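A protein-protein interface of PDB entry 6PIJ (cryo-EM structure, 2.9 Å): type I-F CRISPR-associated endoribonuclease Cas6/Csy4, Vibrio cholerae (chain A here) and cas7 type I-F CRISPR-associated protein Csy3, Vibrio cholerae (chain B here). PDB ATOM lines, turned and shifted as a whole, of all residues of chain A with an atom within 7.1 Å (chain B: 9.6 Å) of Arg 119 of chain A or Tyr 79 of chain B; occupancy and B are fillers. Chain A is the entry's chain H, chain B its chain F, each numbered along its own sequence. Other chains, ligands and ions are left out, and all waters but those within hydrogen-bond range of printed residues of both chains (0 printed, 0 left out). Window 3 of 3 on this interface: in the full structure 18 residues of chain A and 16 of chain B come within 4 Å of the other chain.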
ATOM      1  N   ALA A 112      19.527  -3.203 -15.721  1.00  0.00           N
ATOM      2  CA  ALA A 112      19.370  -2.838 -14.292  1.00  0.00           C
ATOM      3  C   ALA A 112      18.027  -3.369 -13.772  1.00  0.00           C
ATOM      4  O   ALA A 112      18.017  -4.014 -12.701  1.00  0.00           O
ATOM      5  CB  ALA A 112      19.467  -1.340 -14.129  1.00  0.00           C
ATOM      6  N   GLY A 113      16.947  -3.104 -14.517  1.00  0.00           N
ATOM      7  CA  GLY A 113      15.576  -3.580 -14.244  1.00  0.00           C
ATOM      8  C   GLY A 113      15.502  -5.094 -14.110  1.00  0.00           C
ATOM      9  O   GLY A 113      14.903  -5.565 -13.112  1.00  0.00           O
ATOM     10  N   LEU A 114      16.088  -5.830 -15.065  1.00  0.00           N
ATOM     11  CA  LEU A 114      16.143  -7.322 -15.045  1.00  0.00           C
ATOM     12  C   LEU A 114      16.865  -7.785 -13.770  1.00  0.00           C
ATOM     13  O   LEU A 114      16.291  -8.626 -13.037  1.00  0.00           O
ATOM     14  CB  LEU A 114      16.843  -7.844 -16.308  1.00  0.00           C
ATOM     15  CG  LEU A 114      17.137  -9.347 -16.345  1.00  0.00           C
ATOM     16  CD1 LEU A 114      15.875 -10.170 -16.121  1.00  0.00           C
ATOM     17  CD2 LEU A 114      17.797  -9.741 -17.657  1.00  0.00           C
ATOM     18  N   ALA A 115      18.064  -7.244 -13.516  1.00  0.00           N
ATOM     19  CA  ALA A 115      18.889  -7.521 -12.312  1.00  0.00           C
ATOM     20  C   ALA A 115      18.052  -7.282 -11.047  1.00  0.00           C
ATOM     21  O   ALA A 115      18.037  -8.178 -10.172  1.00  0.00           O
ATOM     22  CB  ALA A 115      20.135  -6.667 -12.318  1.00  0.00           C
ATOM     23  N   ARG A 116      17.367  -6.133 -10.979  1.00  0.00           N
ATOM     24  CA  ARG A 116      16.468  -5.740  -9.855  1.00  0.00           C
ATOM     25  C   ARG A 116      15.364  -6.794  -9.684  1.00  0.00           C
ATOM     26  O   ARG A 116      15.108  -7.195  -8.527  1.00  0.00           O
ATOM     27  CB  ARG A 116      15.848  -4.360 -10.098  1.00  0.00           C
ATOM     28  CG  ARG A 116      15.591  -3.562  -8.827  1.00  0.00           C
ATOM     29  CD  ARG A 116      14.978  -2.200  -9.103  1.00  0.00           C
ATOM     30  NE  ARG A 116      15.742  -1.466 -10.112  1.00  0.00           N
ATOM     31  CZ  ARG A 116      15.331  -1.134 -11.341  1.00  0.00           C
ATOM     32  NH1 ARG A 116      16.153  -0.473 -12.140  1.00  0.00           N
ATOM     33  NH2 ARG A 116      14.113  -1.428 -11.773  1.00  0.00           N
ATOM     34  N   LYS A 117      14.744  -7.220 -10.794  1.00  0.00           N
ATOM     35  CA  LYS A 117      13.649  -8.231 -10.816  1.00  0.00           C
ATOM     36  C   LYS A 117      14.176  -9.573 -10.288  1.00  0.00           C
ATOM     37  O   LYS A 117      13.539 -10.121  -9.363  1.00  0.00           O
ATOM     38  CB  LYS A 117      13.070  -8.381 -12.227  1.00  0.00           C
ATOM     39  CG  LYS A 117      11.748  -9.134 -12.311  1.00  0.00           C
ATOM     40  CD  LYS A 117      11.279  -9.383 -13.729  1.00  0.00           C
ATOM     41  CE  LYS A 117      12.066 -10.467 -14.434  1.00  0.00           C
ATOM     42  NZ  LYS A 117      11.474 -10.807 -15.750  1.00  0.00           N
ATOM     43  N   ILE A 118      15.295 -10.067 -10.833  1.00  0.00           N
ATOM     44  CA  ILE A 118      15.911 -11.372 -10.424  1.00  0.00           C
ATOM     45  C   ILE A 118      16.263 -11.306  -8.929  1.00  0.00           C
ATOM     46  O   ILE A 118      16.000 -12.306  -8.224  1.00  0.00           O
ATOM     47  CB  ILE A 118      17.130 -11.743 -11.302  1.00  0.00           C
ATOM     48  CG1 ILE A 118      16.734 -11.951 -12.767  1.00  0.00           C
ATOM     49  CG2 ILE A 118      17.851 -12.972 -10.753  1.00  0.00           C
ATOM     50  CD1 ILE A 118      17.901 -12.169 -13.705  1.00  0.00           C
ATOM     51  N   ARG A 119      16.817 -10.176  -8.467  1.00  0.00           N
ATOM     52  CA  ARG A 119      17.237  -9.960  -7.052  1.00  0.00           C
ATOM     53  C   ARG A 119      16.025 -10.057  -6.117  1.00  0.00           C
ATOM     54  O   ARG A 119      16.177 -10.654  -5.031  1.00  0.00           O
ATOM     55  CB  ARG A 119      17.927  -8.603  -6.878  1.00  0.00           C
ATOM     56  CG  ARG A 119      18.799  -8.502  -5.633  1.00  0.00           C
ATOM     57  CD  ARG A 119      19.270  -7.091  -5.328  1.00  0.00           C
ATOM     58  NE  ARG A 119      19.536  -6.308  -6.535  1.00  0.00           N
ATOM     59  CZ  ARG A 119      19.308  -5.001  -6.694  1.00  0.00           C
ATOM     60  NH1 ARG A 119      19.596  -4.427  -7.851  1.00  0.00           N
ATOM     61  NH2 ARG A 119      18.791  -4.266  -5.721  1.00  0.00           N
ATOM     62  N   ARG A 120      14.881  -9.483  -6.511  1.00  0.00           N
ATOM     63  CA  ARG A 120      13.611  -9.549  -5.735  1.00  0.00           C
ATOM     64  C   ARG A 120      13.138 -11.007  -5.674  1.00  0.00           C
ATOM     65  O   ARG A 120      12.953 -11.518  -4.544  1.00  0.00           O
ATOM     66  CB  ARG A 120      12.531  -8.645  -6.341  1.00  0.00           C
ATOM     67  CG  ARG A 120      11.198  -8.734  -5.615  1.00  0.00           C
ATOM     68  CD  ARG A 120      10.361  -7.470  -5.674  1.00  0.00           C
ATOM     69  NE  ARG A 120       9.374  -7.463  -4.600  1.00  0.00           N
ATOM     70  CZ  ARG A 120       8.275  -8.218  -4.553  1.00  0.00           C
ATOM     71  NH1 ARG A 120       7.455  -8.120  -3.518  1.00  0.00           N
ATOM     72  NH2 ARG A 120       7.977  -9.057  -5.530  1.00  0.00           N
ATOM     73  N   LEU A 121      12.979 -11.650  -6.839  1.00  0.00           N
ATOM     74  CA  LEU A 121      12.583 -13.083  -6.969  1.00  0.00           C
ATOM     75  C   LEU A 121      13.522 -13.972  -6.137  1.00  0.00           C
ATOM     76  O   LEU A 121      13.026 -14.972  -5.582  1.00  0.00           O
ATOM     77  CB  LEU A 121      12.581 -13.503  -8.445  1.00  0.00           C
ATOM     78  CG  LEU A 121      11.238 -13.373  -9.165  1.00  0.00           C
ATOM     79  CD1 LEU A 121      10.822 -11.916  -9.306  1.00  0.00           C
ATOM     80  CD2 LEU A 121      11.286 -14.041 -10.531  1.00  0.00           C
ATOM     81  N   GLU A 122      14.815 -13.626  -6.050  1.00  0.00           N
ATOM     82  CA  GLU A 122      15.817 -14.342  -5.208  1.00  0.00           C
ATOM     83  C   GLU A 122      15.511 -14.116  -3.721  1.00  0.00           C
ATOM     84  O   GLU A 122      15.692 -15.073  -2.941  1.00  0.00           O
ATOM     85  CB  GLU A 122      17.248 -13.913  -5.545  1.00  0.00           C
ATOM     86  CG  GLU A 122      18.310 -14.887  -5.052  1.00  0.00           C
ATOM     87  CD  GLU A 122      18.381 -16.213  -5.793  1.00  0.00           C
ATOM     88  OE1 GLU A 122      18.284 -16.206  -7.036  1.00  0.00           O
ATOM     89  OE2 GLU A 122      18.534 -17.255  -5.123  1.00  0.00           O
ATOM     90  N   LYS A 123      15.075 -12.907  -3.345  1.00  0.00           N
ATOM     91  CA  LYS A 123      14.780 -12.530  -1.934  1.00  0.00           C
ATOM     92  C   LYS A 123      13.531 -13.281  -1.460  1.00  0.00           C
ATOM     93  O   LYS A 123      13.610 -13.930  -0.396  1.00  0.00           O
ATOM     94  CB  LYS A 123      14.605 -11.013  -1.790  1.00  0.00           C
ATOM     95  CG  LYS A 123      14.796 -10.466  -0.380  1.00  0.00           C
ATOM     96  CD  LYS A 123      13.550 -10.507   0.483  1.00  0.00           C
ATOM     97  CE  LYS A 123      13.767  -9.915   1.858  1.00  0.00           C
ATOM     98  NZ  LYS A 123      12.509  -9.865   2.640  1.00  0.00           N
ATOM     99  N   ARG A 124      12.437 -13.207  -2.228  1.00  0.00           N
ATOM    100  CA  ARG A 124      11.127 -13.825  -1.875  1.00  0.00           C
ATOM    101  C   ARG A 124      10.962 -15.172  -2.600  1.00  0.00           C
ATOM    102  O   ARG A 124       9.841 -15.467  -3.068  1.00  0.00           O
ATOM    103  CB  ARG A 124       9.979 -12.841  -2.127  1.00  0.00           C
ATOM    104  CG  ARG A 124       9.799 -12.393  -3.571  1.00  0.00           C
ATOM    105  CD  ARG A 124       8.338 -12.090  -3.834  1.00  0.00           C
ATOM    106  NE  ARG A 124       7.536 -13.310  -3.844  1.00  0.00           N
ATOM    107  CZ  ARG A 124       6.219 -13.381  -3.640  1.00  0.00           C
ATOM    108  NH1 ARG A 124       5.616 -14.559  -3.670  1.00  0.00           N
ATOM    109  NH2 ARG A 124       5.502 -12.295  -3.397  1.00  0.00           N
ATOM    110  N   PHE A 132      17.302 -21.407  -6.228  1.00  0.00           N
ATOM    111  CA  PHE A 132      17.108 -21.492  -7.702  1.00  0.00           C
ATOM    112  C   PHE A 132      18.242 -20.767  -8.441  1.00  0.00           C
ATOM    113  O   PHE A 132      18.642 -19.663  -8.013  1.00  0.00           O
ATOM    114  CB  PHE A 132      15.725 -20.959  -8.095  1.00  0.00           C
ATOM    115  CG  PHE A 132      15.538 -19.470  -7.948  1.00  0.00           C
ATOM    116  CD1 PHE A 132      15.246 -18.898  -6.719  1.00  0.00           C
ATOM    117  CD2 PHE A 132      15.648 -18.638  -9.049  1.00  0.00           C
ATOM    118  CE1 PHE A 132      15.074 -17.528  -6.602  1.00  0.00           C
ATOM    119  CE2 PHE A 132      15.478 -17.268  -8.933  1.00  0.00           C
ATOM    120  CZ  PHE A 132      15.191 -16.714  -7.707  1.00  0.00           C
ATOM    121  N   ASP A 133      18.742 -21.391  -9.514  1.00  0.00           N
ATOM    122  CA  ASP A 133      19.901 -20.921 -10.323  1.00  0.00           C
ATOM    123  C   ASP A 133      19.595 -19.543 -10.907  1.00  0.00           C
ATOM    124  O   ASP A 133      18.608 -19.393 -11.627  1.00  0.00           O
ATOM    125  CB  ASP A 133      20.243 -21.899 -11.453  1.00  0.00           C
ATOM    126  CG  ASP A 133      21.156 -23.046 -11.047  1.00  0.00           C
ATOM    127  OD1 ASP A 133      21.167 -23.401  -9.850  1.00  0.00           O
ATOM    128  OD2 ASP A 133      21.850 -23.579 -11.935  1.00  0.00           O
ATOM    129  N   PRO A 134      20.412 -18.499 -10.624  1.00  0.00           N
ATOM    130  CA  PRO A 134      20.391 -17.276 -11.430  1.00  0.00           C
ATOM    131  C   PRO A 134      20.931 -17.492 -12.857  1.00  0.00           C
ATOM    132  O   PRO A 134      20.728 -16.620 -13.683  1.00  0.00           O
ATOM    133  CB  PRO A 134      21.272 -16.297 -10.636  1.00  0.00           C
ATOM    134  CG  PRO A 134      22.190 -17.184  -9.827  1.00  0.00           C
ATOM    135  CD  PRO A 134      21.364 -18.409  -9.502  1.00  0.00           C
ATOM    136  N   SER A 135      21.603 -18.627 -13.102  1.00  0.00           N
ATOM    137  CA  SER A 135      22.074 -19.104 -14.432  1.00  0.00           C
ATOM    138  C   SER A 135      20.913 -19.215 -15.429  1.00  0.00           C
ATOM    139  O   SER A 135      21.127 -18.868 -16.608  1.00  0.00           O
ATOM    140  CB  SER A 135      22.789 -20.424 -14.306  1.00  0.00           C
ATOM    141  OG  SER A 135      23.887 -20.324 -13.410  1.00  0.00           O
ATOM    142  N   PHE A 137      18.237 -17.492 -16.071  1.00  0.00           N
ATOM    143  CA  PHE A 137      17.542 -16.189 -16.270  1.00  0.00           C
ATOM    144  C   PHE A 137      18.367 -15.320 -17.224  1.00  0.00           C
ATOM    145  O   PHE A 137      19.182 -14.497 -16.754  1.00  0.00           O
ATOM    146  CB  PHE A 137      17.302 -15.479 -14.937  1.00  0.00           C
ATOM    147  CG  PHE A 137      16.301 -16.178 -14.057  1.00  0.00           C
ATOM    148  CD1 PHE A 137      14.942 -15.922 -14.172  1.00  0.00           C
ATOM    149  CD2 PHE A 137      16.721 -17.126 -13.139  1.00  0.00           C
ATOM    150  CE1 PHE A 137      14.026 -16.588 -13.371  1.00  0.00           C
ATOM    151  CE2 PHE A 137      15.805 -17.794 -12.345  1.00  0.00           C
ATOM    152  CZ  PHE A 137      14.459 -17.524 -12.457  1.00  0.00           C
ATOM    153  N   VAL B  21      31.090 -15.954 -19.230  1.00  0.00           N
ATOM    154  CA  VAL B  21      30.577 -15.756 -17.843  1.00  0.00           C
ATOM    155  C   VAL B  21      30.897 -17.040 -17.072  1.00  0.00           C
ATOM    156  O   VAL B  21      30.311 -18.092 -17.421  1.00  0.00           O
ATOM    157  CB  VAL B  21      29.070 -15.433 -17.808  1.00  0.00           C
ATOM    158  CG1 VAL B  21      28.612 -15.042 -16.411  1.00  0.00           C
ATOM    159  CG2 VAL B  21      28.692 -14.347 -18.804  1.00  0.00           C
ATOM    160  N   VAL B  22      31.811 -16.959 -16.099  1.00  0.00           N
ATOM    161  CA  VAL B  22      32.170 -18.087 -15.187  1.00  0.00           C
ATOM    162  C   VAL B  22      31.392 -17.884 -13.882  1.00  0.00           C
ATOM    163  O   VAL B  22      31.408 -16.753 -13.347  1.00  0.00           O
ATOM    164  CB  VAL B  22      33.693 -18.245 -14.976  1.00  0.00           C
ATOM    165  CG1 VAL B  22      34.409 -16.943 -14.649  1.00  0.00           C
ATOM    166  CG2 VAL B  22      34.017 -19.300 -13.927  1.00  0.00           C
ATOM    167  N   TRP B  23      30.710 -18.941 -13.423  1.00  0.00           N
ATOM    168  CA  TRP B  23      29.689 -18.904 -12.341  1.00  0.00           C
ATOM    169  C   TRP B  23      30.311 -19.336 -11.013  1.00  0.00           C
ATOM    170  O   TRP B  23      31.379 -19.949 -11.004  1.00  0.00           O
ATOM    171  CB  TRP B  23      28.492 -19.783 -12.726  1.00  0.00           C
ATOM    172  CG  TRP B  23      27.707 -19.244 -13.882  1.00  0.00           C
ATOM    173  CD1 TRP B  23      27.853 -19.564 -15.200  1.00  0.00           C
ATOM    174  CD2 TRP B  23      26.654 -18.265 -13.823  1.00  0.00           C
ATOM    175  NE1 TRP B  23      26.962 -18.858 -15.962  1.00  0.00           N
ATOM    176  CE2 TRP B  23      26.213 -18.053 -15.147  1.00  0.00           C
ATOM    177  CE3 TRP B  23      26.040 -17.553 -12.786  1.00  0.00           C
ATOM    178  CZ2 TRP B  23      25.188 -17.158 -15.457  1.00  0.00           C
ATOM    179  CZ3 TRP B  23      25.028 -16.668 -13.092  1.00  0.00           C
ATOM    180  CH2 TRP B  23      24.610 -16.473 -14.410  1.00  0.00           C
ATOM    181  N   PRO B  24      29.661 -19.050  -9.855  1.00  0.00           N
ATOM    182  CA  PRO B  24      30.138 -19.530  -8.553  1.00  0.00           C
ATOM    183  C   PRO B  24      30.314 -21.055  -8.428  1.00  0.00           C
ATOM    184  O   PRO B  24      30.939 -21.476  -7.471  1.00  0.00           O
ATOM    185  CB  PRO B  24      29.048 -19.067  -7.572  1.00  0.00           C
ATOM    186  CG  PRO B  24      28.431 -17.865  -8.249  1.00  0.00           C
ATOM    187  CD  PRO B  24      28.455 -18.212  -9.722  1.00  0.00           C
ATOM    188  N   ARG B  27      31.719 -23.151 -13.447  1.00  0.00           N
ATOM    189  CA  ARG B  27      31.340 -23.545 -14.830  1.00  0.00           C
ATOM    190  C   ARG B  27      31.228 -22.253 -15.647  1.00  0.00           C
ATOM    191  O   ARG B  27      30.848 -21.215 -15.058  1.00  0.00           O
ATOM    192  CB  ARG B  27      30.058 -24.391 -14.845  1.00  0.00           C
ATOM    193  CG  ARG B  27      28.759 -23.614 -15.022  1.00  0.00           C
ATOM    194  CD  ARG B  27      27.562 -24.521 -15.237  1.00  0.00           C
ATOM    195  NE  ARG B  27      26.309 -23.836 -14.940  1.00  0.00           N
ATOM    196  CZ  ARG B  27      25.810 -23.623 -13.720  1.00  0.00           C
ATOM    197  NH1 ARG B  27      26.449 -24.040 -12.637  1.00  0.00           N
ATOM    198  NH2 ARG B  27      24.660 -22.983 -13.589  1.00  0.00           N
ATOM    199  N   LEU B  31      29.140 -15.530 -22.799  1.00  0.00           N
ATOM    200  CA  LEU B  31      28.473 -14.229 -22.517  1.00  0.00           C
ATOM    201  C   LEU B  31      27.577 -13.881 -23.710  1.00  0.00           C
ATOM    202  O   LEU B  31      28.101 -13.832 -24.834  1.00  0.00           O
ATOM    203  CB  LEU B  31      29.539 -13.151 -22.275  1.00  0.00           C
ATOM    204  CG  LEU B  31      29.030 -11.718 -22.103  1.00  0.00           C
ATOM    205  CD1 LEU B  31      28.346 -11.534 -20.757  1.00  0.00           C
ATOM    206  CD2 LEU B  31      30.171 -10.723 -22.261  1.00  0.00           C
ATOM    207  N   HIS B  76      25.603  -6.683 -20.399  1.00  0.00           N
ATOM    208  CA  HIS B  76      25.958  -6.600 -18.957  1.00  0.00           C
ATOM    209  C   HIS B  76      26.348  -7.989 -18.444  1.00  0.00           C
ATOM    210  O   HIS B  76      26.079  -8.982 -19.153  1.00  0.00           O
ATOM    211  CB  HIS B  76      24.796  -6.003 -18.154  1.00  0.00           C
ATOM    212  CG  HIS B  76      24.507  -4.578 -18.487  1.00  0.00           C
ATOM    213  ND1 HIS B  76      23.699  -4.218 -19.547  1.00  0.00           N
ATOM    214  CD2 HIS B  76      24.915  -3.427 -17.911  1.00  0.00           C
ATOM    215  CE1 HIS B  76      23.617  -2.904 -19.607  1.00  0.00           C
ATOM    216  NE2 HIS B  76      24.356  -2.395 -18.614  1.00  0.00           N
ATOM    217  N   VAL B  77      26.952  -8.048 -17.254  1.00  0.00           N
ATOM    218  CA  VAL B  77      27.294  -9.321 -16.550  1.00  0.00           C
ATOM    219  C   VAL B  77      26.010  -9.816 -15.887  1.00  0.00           C
ATOM    220  O   VAL B  77      25.394  -9.067 -15.131  1.00  0.00           O
ATOM    221  CB  VAL B  77      28.432  -9.137 -15.525  1.00  0.00           C
ATOM    222  CG1 VAL B  77      28.953 -10.475 -15.019  1.00  0.00           C
ATOM    223  CG2 VAL B  77      29.581  -8.302 -16.080  1.00  0.00           C
ATOM    224  N   PRO B  78      25.552 -11.066 -16.143  1.00  0.00           N
ATOM    225  CA  PRO B  78      24.277 -11.540 -15.599  1.00  0.00           C
ATOM    226  C   PRO B  78      24.343 -11.683 -14.071  1.00  0.00           C
ATOM    227  O   PRO B  78      25.422 -11.935 -13.558  1.00  0.00           O
ATOM    228  CB  PRO B  78      24.081 -12.903 -16.277  1.00  0.00           C
ATOM    229  CG  PRO B  78      25.492 -13.371 -16.531  1.00  0.00           C
ATOM    230  CD  PRO B  78      26.241 -12.112 -16.916  1.00  0.00           C
ATOM    231  N   TYR B  79      23.203 -11.515 -13.393  1.00  0.00           N
ATOM    232  CA  TYR B  79      23.103 -11.491 -11.909  1.00  0.00           C
ATOM    233  C   TYR B  79      23.633 -12.812 -11.336  1.00  0.00           C
ATOM    234  O   TYR B  79      23.327 -13.878 -11.901  1.00  0.00           O
ATOM    235  CB  TYR B  79      21.669 -11.229 -11.442  1.00  0.00           C
ATOM    236  CG  TYR B  79      21.563 -11.071  -9.947  1.00  0.00           C
ATOM    237  CD1 TYR B  79      21.956  -9.895  -9.326  1.00  0.00           C
ATOM    238  CD2 TYR B  79      21.128 -12.115  -9.143  1.00  0.00           C
ATOM    239  CE1 TYR B  79      21.892  -9.748  -7.949  1.00  0.00           C
ATOM    240  CE2 TYR B  79      21.057 -11.984  -7.764  1.00  0.00           C
ATOM    241  CZ  TYR B  79      21.441 -10.797  -7.165  1.00  0.00           C
ATOM    242  OH  TYR B  79      21.377 -10.669  -5.807  1.00  0.00           O
ATOM    243  N   GLY B  80      24.422 -12.727 -10.259  1.00  0.00           N
ATOM    244  CA  GLY B  80      24.960 -13.880  -9.510  1.00  0.00           C
ATOM    245  C   GLY B  80      26.066 -14.614 -10.254  1.00  0.00           C
ATOM    246  O   GLY B  80      26.208 -15.831 -10.020  1.00  0.00           O
ATOM    247  N   ALA B  81      26.833 -13.911 -11.098  1.00  0.00           N
ATOM    248  CA  ALA B  81      27.999 -14.442 -11.846  1.00  0.00           C
ATOM    249  C   ALA B  81      29.280 -14.164 -11.047  1.00  0.00           C
ATOM    250  O   ALA B  81      29.368 -13.077 -10.438  1.00  0.00           O
ATOM    251  CB  ALA B  81      28.064 -13.821 -13.220  1.00  0.00           C
ATOM    252  N   SER B  82      30.232 -15.105 -11.056  1.00  0.00           N
ATOM    253  CA  SER B  82      31.516 -15.011 -10.311  1.00  0.00           C
ATOM    254  C   SER B  82      32.401 -13.935 -10.951  1.00  0.00           C
ATOM    255  O   SER B  82      32.715 -12.948 -10.256  1.00  0.00           O
ATOM    256  CB  SER B  82      32.226 -16.342 -10.238  1.00  0.00           C
ATOM    257  OG  SER B  82      33.386 -16.255  -9.421  1.00  0.00           O
ATOM    258  N   HIS B  83      32.769 -14.115 -12.225  1.00  0.00           N
ATOM    259  CA  HIS B  83      33.600 -13.156 -13.006  1.00  0.00           C
ATOM    260  C   HIS B  83      33.515 -13.462 -14.510  1.00  0.00           C
ATOM    261  O   HIS B  83      32.739 -14.364 -14.891  1.00  0.00           O
ATOM    262  CB  HIS B  83      35.038 -13.140 -12.457  1.00  0.00           C
ATOM    263  CG  HIS B  83      35.747 -14.452 -12.493  1.00  0.00           C
ATOM    264  ND1 HIS B  83      35.479 -15.465 -11.592  1.00  0.00           N
ATOM    265  CD2 HIS B  83      36.745 -14.902 -13.285  1.00  0.00           C
ATOM    266  CE1 HIS B  83      36.267 -16.491 -11.843  1.00  0.00           C
ATOM    267  NE2 HIS B  83      37.056 -16.170 -12.875  1.00  0.00           N
ATOM    268  N   ILE B  84      34.253 -12.697 -15.327  1.00  0.00           N
ATOM    269  CA  ILE B  84      34.332 -12.831 -16.814  1.00  0.00           C
ATOM    270  C   ILE B  84      35.712 -13.394 -17.183  1.00  0.00           C
ATOM    271  O   ILE B  84      36.700 -12.965 -16.562  1.00  0.00           O
ATOM    272  CB  ILE B  84      34.061 -11.467 -17.491  1.00  0.00           C
ATOM    273  CG1 ILE B  84      32.635 -10.969 -17.229  1.00  0.00           C
ATOM    274  CG2 ILE B  84      34.377 -11.504 -18.981  1.00  0.00           C
ATOM    275  CD1 ILE B  84      31.540 -11.865 -17.774  1.00  0.00           C
ATOM    276  N   PRO B 215      32.178  -5.110 -10.900  1.00  0.00           N
ATOM    277  CA  PRO B 215      31.033  -4.907 -10.012  1.00  0.00           C
ATOM    278  C   PRO B 215      29.751  -5.548 -10.572  1.00  0.00           C
ATOM    279  O   PRO B 215      29.679  -5.772 -11.768  1.00  0.00           O
ATOM    280  CB  PRO B 215      30.889  -3.377  -9.909  1.00  0.00           C
ATOM    281  CG  PRO B 215      31.636  -2.835 -11.109  1.00  0.00           C
ATOM    282  CD  PRO B 215      32.739  -3.836 -11.377  1.00  0.00           C
ATOM    283  N   THR B 216      28.789  -5.840  -9.689  1.00  0.00           N
ATOM    284  CA  THR B 216      27.495  -6.509 -10.007  1.00  0.00           C
ATOM    285  C   THR B 216      26.781  -5.755 -11.140  1.00  0.00           C
ATOM    286  O   THR B 216      26.616  -4.524 -11.016  1.00  0.00           O
ATOM    287  CB  THR B 216      26.614  -6.659  -8.756  1.00  0.00           C
ATOM    288  OG1 THR B 216      25.437  -7.374  -9.136  1.00  0.00           O
ATOM    289  CG2 THR B 216      26.220  -5.346  -8.110  1.00  0.00           C
ATOM    290  N   ASN B 217      26.410  -6.473 -12.208  1.00  0.00           N
ATOM    291  CA  ASN B 217      25.649  -5.954 -13.378  1.00  0.00           C
ATOM    292  C   ASN B 217      26.419  -4.779 -14.002  1.00  0.00           C
ATOM    293  O   ASN B 217      25.832  -3.686 -14.148  1.00  0.00           O
ATOM    294  CB  ASN B 217      24.211  -5.602 -12.981  1.00  0.00           C
ATOM    295  CG  ASN B 217      23.293  -5.424 -14.172  1.00  0.00           C
ATOM    296  OD1 ASN B 217      22.971  -4.300 -14.554  1.00  0.00           O
ATOM    297  ND2 ASN B 217      22.874  -6.526 -14.772  1.00  0.00           N
ATOM    298  N   ALA B 218      27.694  -5.000 -14.344  1.00  0.00           N
ATOM    299  CA  ALA B 218      28.591  -4.010 -14.990  1.00  0.00           C
ATOM    300  C   ALA B 218      28.485  -4.141 -16.512  1.00  0.00           C
ATOM    301  O   ALA B 218      28.248  -5.264 -16.994  1.00  0.00           O
ATOM    302  CB  ALA B 218      30.014  -4.206 -14.529  1.00  0.00           C
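OD2 of Asp 133 of chain A is in salt-bridge range of NH2 of Arg 27 of chain B, 3.3 Å away. The guanidinium group (NH2) of Arg 27 of chain B lies within hydrogen-bond range of the side-chain hydroxyl (OG) of Ser 135 of chain A (2.8 Å).
Among the printed residues, pairs that only touch across the chains: Ala 112 of chain A with Asn 217 of chain B, Ala 115 of chain A with Asn 217 of chain B, Ile 118 of chain A with Tyr 79 of chain B, Arg 119 of chain A with Tyr 79 of chain B, Pro 134 of chain A with Trp 23 of chain B, Pro 134 of chain A with Tyr 79 of chain B and Ser 135 of chain A with Trp 23 of chain B.
Of the printed residues of chain B, Ala 115 of chain A touches Asn 217 (3.7 Å). Of chain B, only Tyr 79 (3.4 Å) comes within 4 Å of Arg 119 of chain A. Of the printed residues of chain B, Pro 134 of chain A touches Trp 23 (3.95 Å) and Tyr 79 (3.4 Å). Of the printed residues of chain A, Trp 23 of chain B touches Pro 134 and Ser 135. Printed residues of chain A within 4 Å of Arg 27 of chain B: Asp 133 (3.3 Å) and Ser 135 (2.8 Å). Tyr 79 of chain B touches just these residues of chain A: Ile 118, Arg 119 and Pro 134. Printed residues of chain A within 4 Å of Asn 217 of chain B: Ala 112 and Ala 115. The nearest residue of chain B that does not touch Arg 119 of chain A is Thr 216 of chain B (6.5 Å). The nearest printed residue of chain A that does not touch Asn 217 of chain B is Gly 113 of chain A (6.1 Å).
Of the 18 printed residues of chain A, 7 touch a printed residue of chain B. Among the printed residues, 9 pairs touch across the chains.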
